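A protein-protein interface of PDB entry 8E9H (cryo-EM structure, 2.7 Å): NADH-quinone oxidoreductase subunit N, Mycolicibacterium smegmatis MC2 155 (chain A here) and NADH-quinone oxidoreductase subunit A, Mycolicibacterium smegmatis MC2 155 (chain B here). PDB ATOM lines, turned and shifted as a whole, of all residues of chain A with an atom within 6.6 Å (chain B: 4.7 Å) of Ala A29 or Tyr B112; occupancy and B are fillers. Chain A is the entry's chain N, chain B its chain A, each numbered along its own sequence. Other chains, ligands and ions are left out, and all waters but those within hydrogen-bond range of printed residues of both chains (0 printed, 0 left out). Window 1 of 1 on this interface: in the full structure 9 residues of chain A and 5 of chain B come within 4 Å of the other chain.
The side-chain carboxylate (OE1) of Glu A28 is in salt-bridge range of the guanidinium group (NH1) of Arg B116 (3.1 Å). O of Ala A29 lies within hydrogen-bond range of NH1 of Arg B115, 2.9 Å away. The side-chain carboxylate (OE2) of Glu A143 lies within hydrogen-bond range of the side-chain hydroxyl (OH) of Tyr B112 (2.7 Å). OE2 of Glu A143 is in salt-bridge range of NH2 of Arg B116, 2.7 Å away.
The side-chain carboxylate (OE1) of Glu A28 is in salt-bridge range of the guanidinium group (NE) of Arg A36 (3.9 Å).
Val A25 touches Val B108 (CG1 to CG1, 3.5 Å). Tyr B112 touches Val A25 (CB to CG1, 3.9 Å). Val B108 touches Leu A26. Glu A28 touches Tyr B112. CB of Ala A29 touches CA of Tyr B112, 3.5 Å away. Arg B115 touches Leu A30 (NH1 to CA, 3.6 Å).
Of chain B, only Tyr B112 (3.5 Å) and Arg B115 (2.9 Å) come within 4 Å of Ala A29. Printed residues of chain B within 4 Å of Glu A28: Tyr B112 and Arg B116. Printed residues of chain B within 4 Å of Leu A30: Arg B115 (3.6 Å). Printed residues of chain A within 4 Å of Arg B115: Ala A29 (2.9 Å) and Leu A30 (3.6 Å). Printed residues of chain B within 4 Å of Val A25: Val B108 (3.5 Å) and Tyr B112 (3.9 Å). Printed residues of chain A within 4 Å of Val B108: Val A25 (3.5 Å) and Leu A26 (3.8 Å). The nearest printed residue of chain B that does not touch Glu A143 is Val B113 (8.4 Å).
Of the 11 printed residues of chain A, 6 touch a printed residue of chain B. Printed residues of chain B that touch a printed residue of chain A: Val B108, Tyr B112, Arg B115 and Arg B116. Among the printed residues, 10 pairs touch across the chains. Among the printed residues, Asp or Glu carboxylates within 4 Å of a Lys or Arg side-chain nitrogen of the other chain: Glu A28 with Arg B116 and Glu A143 with Arg B116.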
ATOM      1  N   GLY A  24     -26.233 -14.837  17.610  1.00  0.00           N
ATOM      2  CA  GLY A  24     -27.531 -14.330  18.017  1.00  0.00           C
ATOM      3  C   GLY A  24     -27.524 -12.826  18.194  1.00  0.00           C
ATOM      4  O   GLY A  24     -28.498 -12.144  17.867  1.00  0.00           O
ATOM      5  N   VAL A  25     -26.425 -12.287  18.722  1.00  0.00           N
ATOM      6  CA  VAL A  25     -26.300 -10.836  18.783  1.00  0.00           C
ATOM      7  C   VAL A  25     -26.299 -10.249  17.380  1.00  0.00           C
ATOM      8  O   VAL A  25     -26.893  -9.193  17.140  1.00  0.00           O
ATOM      9  CB  VAL A  25     -25.037 -10.434  19.561  1.00  0.00           C
ATOM     10  CG1 VAL A  25     -24.841  -8.933  19.503  1.00  0.00           C
ATOM     11  CG2 VAL A  25     -25.145 -10.896  20.996  1.00  0.00           C
ATOM     12  N   LEU A  26     -25.642 -10.917  16.432  1.00  0.00           N
ATOM     13  CA  LEU A  26     -25.683 -10.450  15.050  1.00  0.00           C
ATOM     14  C   LEU A  26     -27.104 -10.475  14.505  1.00  0.00           C
ATOM     15  O   LEU A  26     -27.507  -9.574  13.763  1.00  0.00           O
ATOM     16  CB  LEU A  26     -24.771 -11.302  14.171  1.00  0.00           C
ATOM     17  CG  LEU A  26     -23.306 -10.882  14.106  1.00  0.00           C
ATOM     18  CD1 LEU A  26     -22.513 -11.887  13.297  1.00  0.00           C
ATOM     19  CD2 LEU A  26     -23.171  -9.495  13.508  1.00  0.00           C
ATOM     20  N   ILE A  27     -27.866 -11.515  14.834  1.00  0.00           N
ATOM     21  CA  ILE A  27     -29.260 -11.570  14.402  1.00  0.00           C
ATOM     22  C   ILE A  27     -30.034 -10.398  14.984  1.00  0.00           C
ATOM     23  O   ILE A  27     -30.808  -9.735  14.283  1.00  0.00           O
ATOM     24  CB  ILE A  27     -29.898 -12.916  14.794  1.00  0.00           C
ATOM     25  CG1 ILE A  27     -29.168 -14.087  14.131  1.00  0.00           C
ATOM     26  CG2 ILE A  27     -31.363 -12.933  14.410  1.00  0.00           C
ATOM     27  CD1 ILE A  27     -28.847 -13.881  12.669  1.00  0.00           C
ATOM     28  N   GLU A  28     -29.839 -10.120  16.272  1.00  0.00           N
ATOM     29  CA  GLU A  28     -30.468  -8.949  16.871  1.00  0.00           C
ATOM     30  C   GLU A  28     -30.081  -7.686  16.120  1.00  0.00           C
ATOM     31  O   GLU A  28     -30.907  -6.786  15.928  1.00  0.00           O
ATOM     32  CB  GLU A  28     -30.064  -8.822  18.339  1.00  0.00           C
ATOM     33  CG  GLU A  28     -30.598  -9.908  19.241  1.00  0.00           C
ATOM     34  CD  GLU A  28     -32.100 -10.047  19.161  1.00  0.00           C
ATOM     35  OE1 GLU A  28     -32.798  -9.015  19.235  1.00  0.00           O
ATOM     36  OE2 GLU A  28     -32.587 -11.190  19.025  1.00  0.00           O
ATOM     37  N   ALA A  29     -28.825  -7.602  15.688  1.00  0.00           N
ATOM     38  CA  ALA A  29     -28.335  -6.381  15.063  1.00  0.00           C
ATOM     39  C   ALA A  29     -28.929  -6.190  13.674  1.00  0.00           C
ATOM     40  O   ALA A  29     -29.617  -5.196  13.414  1.00  0.00           O
ATOM     41  CB  ALA A  29     -26.810  -6.415  14.988  1.00  0.00           C
ATOM     42  N   LEU A  30     -28.683  -7.137  12.769  1.00  0.00           N
ATOM     43  CA  LEU A  30     -28.963  -6.936  11.354  1.00  0.00           C
ATOM     44  C   LEU A  30     -30.029  -7.875  10.802  1.00  0.00           C
ATOM     45  O   LEU A  30     -30.018  -8.156   9.599  1.00  0.00           O
ATOM     46  CB  LEU A  30     -27.676  -7.085  10.535  1.00  0.00           C
ATOM     47  CG  LEU A  30     -26.883  -8.377  10.729  1.00  0.00           C
ATOM     48  CD1 LEU A  30     -27.378  -9.473   9.802  1.00  0.00           C
ATOM     49  CD2 LEU A  30     -25.407  -8.119  10.506  1.00  0.00           C
ATOM     50  N   ALA A  31     -30.941  -8.368  11.635  1.00  0.00           N
ATOM     51  CA  ALA A  31     -32.033  -9.157  11.083  1.00  0.00           C
ATOM     52  C   ALA A  31     -33.354  -8.415  11.233  1.00  0.00           C
ATOM     53  O   ALA A  31     -33.558  -7.713  12.228  1.00  0.00           O
ATOM     54  CB  ALA A  31     -32.137 -10.512  11.782  1.00  0.00           C
ATOM     55  N   PRO A  32     -34.276  -8.538  10.283  1.00  0.00           N
ATOM     56  CA  PRO A  32     -35.563  -7.855  10.424  1.00  0.00           C
ATOM     57  C   PRO A  32     -36.353  -8.406  11.599  1.00  0.00           C
ATOM     58  O   PRO A  32     -36.234  -9.577  11.964  1.00  0.00           O
ATOM     59  CB  PRO A  32     -36.265  -8.138   9.093  1.00  0.00           C
ATOM     60  CG  PRO A  32     -35.643  -9.387   8.603  1.00  0.00           C
ATOM     61  CD  PRO A  32     -34.215  -9.337   9.048  1.00  0.00           C
ATOM     62  N   ARG A  36     -36.628 -12.260  13.518  1.00  0.00           N
ATOM     63  CA  ARG A  36     -35.645 -12.405  14.587  1.00  0.00           C
ATOM     64  C   ARG A  36     -35.923 -13.632  15.444  1.00  0.00           C
ATOM     65  O   ARG A  36     -35.016 -14.431  15.699  1.00  0.00           O
ATOM     66  CB  ARG A  36     -35.609 -11.145  15.448  1.00  0.00           C
ATOM     67  CG  ARG A  36     -34.763 -10.039  14.848  1.00  0.00           C
ATOM     68  CD  ARG A  36     -34.246  -9.083  15.900  1.00  0.00           C
ATOM     69  NE  ARG A  36     -35.258  -8.117  16.302  1.00  0.00           N
ATOM     70  CZ  ARG A  36     -35.435  -6.935  15.728  1.00  0.00           C
ATOM     71  NH1 ARG A  36     -34.705  -6.550  14.695  1.00  0.00           N
ATOM     72  NH2 ARG A  36     -36.375  -6.121  16.199  1.00  0.00           N
ATOM     73  N   GLU A 143     -33.427 -10.354  22.498  1.00  0.00           N
ATOM     74  CA  GLU A 143     -32.126 -10.315  23.152  1.00  0.00           C
ATOM     75  C   GLU A 143     -32.009 -11.350  24.259  1.00  0.00           C
ATOM     76  O   GLU A 143     -30.892 -11.671  24.679  1.00  0.00           O
ATOM     77  CB  GLU A 143     -31.873  -8.925  23.727  1.00  0.00           C
ATOM     78  CG  GLU A 143     -31.540  -7.884  22.687  1.00  0.00           C
ATOM     79  CD  GLU A 143     -32.772  -7.317  22.011  1.00  0.00           C
ATOM     80  OE1 GLU A 143     -33.873  -7.864  22.223  1.00  0.00           O
ATOM     81  OE2 GLU A 143     -32.638  -6.323  21.268  1.00  0.00           O
ATOM     82  N   VAL B 108     -19.331  -6.548  16.789  1.00  0.00           N
ATOM     83  CA  VAL B 108     -20.684  -7.087  16.817  1.00  0.00           C
ATOM     84  C   VAL B 108     -21.510  -6.373  17.871  1.00  0.00           C
ATOM     85  O   VAL B 108     -22.645  -5.961  17.610  1.00  0.00           O
ATOM     86  CB  VAL B 108     -20.653  -8.606  17.062  1.00  0.00           C
ATOM     87  CG1 VAL B 108     -22.036  -9.112  17.419  1.00  0.00           C
ATOM     88  CG2 VAL B 108     -20.124  -9.323  15.838  1.00  0.00           C
ATOM     89  N   ALA B 109     -20.955  -6.199  19.071  1.00  0.00           N
ATOM     90  CA  ALA B 109     -21.684  -5.477  20.111  1.00  0.00           C
ATOM     91  C   ALA B 109     -21.992  -4.055  19.666  1.00  0.00           C
ATOM     92  O   ALA B 109     -23.120  -3.564  19.820  1.00  0.00           O
ATOM     93  CB  ALA B 109     -20.872  -5.457  21.403  1.00  0.00           C
ATOM     94  N   TYR B 110     -20.994  -3.383  19.101  1.00  0.00           N
ATOM     95  CA  TYR B 110     -21.146  -1.996  18.691  1.00  0.00           C
ATOM     96  C   TYR B 110     -22.195  -1.861  17.597  1.00  0.00           C
ATOM     97  O   TYR B 110     -23.008  -0.934  17.609  1.00  0.00           O
ATOM     98  CB  TYR B 110     -19.800  -1.468  18.212  1.00  0.00           C
ATOM     99  CG  TYR B 110     -19.840  -0.026  17.825  1.00  0.00           C
ATOM    100  CD1 TYR B 110     -19.723   0.968  18.779  1.00  0.00           C
ATOM    101  CD2 TYR B 110     -20.029   0.343  16.509  1.00  0.00           C
ATOM    102  CE1 TYR B 110     -19.770   2.287  18.428  1.00  0.00           C
ATOM    103  CE2 TYR B 110     -20.082   1.654  16.151  1.00  0.00           C
ATOM    104  CZ  TYR B 110     -19.953   2.622  17.113  1.00  0.00           C
ATOM    105  OH  TYR B 110     -20.008   3.937  16.744  1.00  0.00           O
ATOM    106  N   ALA B 111     -22.177  -2.776  16.631  1.00  0.00           N
ATOM    107  CA  ALA B 111     -23.139  -2.751  15.539  1.00  0.00           C
ATOM    108  C   ALA B 111     -24.540  -3.036  16.050  1.00  0.00           C
ATOM    109  O   ALA B 111     -25.519  -2.454  15.577  1.00  0.00           O
ATOM    110  CB  ALA B 111     -22.736  -3.765  14.469  1.00  0.00           C
ATOM    111  N   TYR B 112     -24.661  -3.947  17.015  1.00  0.00           N
ATOM    112  CA  TYR B 112     -25.966  -4.185  17.613  1.00  0.00           C
ATOM    113  C   TYR B 112     -26.493  -2.913  18.253  1.00  0.00           C
ATOM    114  O   TYR B 112     -27.661  -2.550  18.081  1.00  0.00           O
ATOM    115  CB  TYR B 112     -25.883  -5.295  18.654  1.00  0.00           C
ATOM    116  CG  TYR B 112     -27.067  -5.283  19.582  1.00  0.00           C
ATOM    117  CD1 TYR B 112     -28.312  -5.692  19.144  1.00  0.00           C
ATOM    118  CD2 TYR B 112     -26.949  -4.828  20.881  1.00  0.00           C
ATOM    119  CE1 TYR B 112     -29.399  -5.673  19.977  1.00  0.00           C
ATOM    120  CE2 TYR B 112     -28.032  -4.804  21.723  1.00  0.00           C
ATOM    121  CZ  TYR B 112     -29.256  -5.226  21.265  1.00  0.00           C
ATOM    122  OH  TYR B 112     -30.345  -5.202  22.099  1.00  0.00           O
ATOM    123  N   VAL B 113     -25.635  -2.220  18.998  1.00  0.00           N
ATOM    124  CA  VAL B 113     -26.050  -0.971  19.632  1.00  0.00           C
ATOM    125  C   VAL B 113     -26.468   0.044  18.579  1.00  0.00           C
ATOM    126  O   VAL B 113     -27.528   0.670  18.674  1.00  0.00           O
ATOM    127  CB  VAL B 113     -24.918  -0.422  20.515  1.00  0.00           C
ATOM    128  CG1 VAL B 113     -25.104   1.061  20.748  1.00  0.00           C
ATOM    129  CG2 VAL B 113     -24.871  -1.169  21.830  1.00  0.00           C
ATOM    130  N   TRP B 114     -25.633   0.220  17.558  1.00  0.00           N
ATOM    131  CA  TRP B 114     -25.857   1.276  16.579  1.00  0.00           C
ATOM    132  C   TRP B 114     -27.109   1.011  15.759  1.00  0.00           C
ATOM    133  O   TRP B 114     -27.975   1.882  15.627  1.00  0.00           O
ATOM    134  CB  TRP B 114     -24.624   1.390  15.684  1.00  0.00           C
ATOM    135  CG  TRP B 114     -24.622   2.544  14.745  1.00  0.00           C
ATOM    136  CD1 TRP B 114     -25.637   3.419  14.510  1.00  0.00           C
ATOM    137  CD2 TRP B 114     -23.533   2.963  13.922  1.00  0.00           C
ATOM    138  NE1 TRP B 114     -25.254   4.351  13.580  1.00  0.00           N
ATOM    139  CE2 TRP B 114     -23.963   4.093  13.205  1.00  0.00           C
ATOM    140  CE3 TRP B 114     -22.237   2.489  13.718  1.00  0.00           C
ATOM    141  CZ2 TRP B 114     -23.143   4.755  12.301  1.00  0.00           C
ATOM    142  CZ3 TRP B 114     -21.427   3.147  12.821  1.00  0.00           C
ATOM    143  CH2 TRP B 114     -21.880   4.267  12.123  1.00  0.00           C
ATOM    144  N   ARG B 115     -27.231  -0.193  15.207  1.00  0.00           N
ATOM    145  CA  ARG B 115     -28.322  -0.473  14.288  1.00  0.00           C
ATOM    146  C   ARG B 115     -29.666  -0.555  14.993  1.00  0.00           C
ATOM    147  O   ARG B 115     -30.702  -0.434  14.334  1.00  0.00           O
ATOM    148  CB  ARG B 115     -28.048  -1.770  13.533  1.00  0.00           C
ATOM    149  CG  ARG B 115     -28.752  -1.837  12.198  1.00  0.00           C
ATOM    150  CD  ARG B 115     -28.194  -2.940  11.330  1.00  0.00           C
ATOM    151  NE  ARG B 115     -28.942  -3.078  10.086  1.00  0.00           N
ATOM    152  CZ  ARG B 115     -30.187  -3.525  10.005  1.00  0.00           C
ATOM    153  NH1 ARG B 115     -30.862  -3.894  11.081  1.00  0.00           N
ATOM    154  NH2 ARG B 115     -30.769  -3.607   8.812  1.00  0.00           N
ATOM    155  N   ARG B 116     -29.677  -0.755  16.308  1.00  0.00           N
ATOM    156  CA  ARG B 116     -30.912  -0.778  17.074  1.00  0.00           C
ATOM    157  C   ARG B 116     -31.207   0.559  17.737  1.00  0.00           C
ATOM    158  O   ARG B 116     -32.004   0.611  18.680  1.00  0.00           O
ATOM    159  CB  ARG B 116     -30.863  -1.890  18.123  1.00  0.00           C
ATOM    160  CG  ARG B 116     -30.848  -3.290  17.535  1.00  0.00           C
ATOM    161  CD  ARG B 116     -32.185  -3.661  16.912  1.00  0.00           C
ATOM    162  NE  ARG B 116     -33.219  -3.892  17.913  1.00  0.00           N
ATOM    163  CZ  ARG B 116     -33.328  -4.995  18.640  1.00  0.00           C
ATOM    164  NH1 ARG B 116     -32.477  -5.999  18.505  1.00  0.00           N
ATOM    165  NH2 ARG B 116     -34.317  -5.097  19.522  1.00  0.00           N
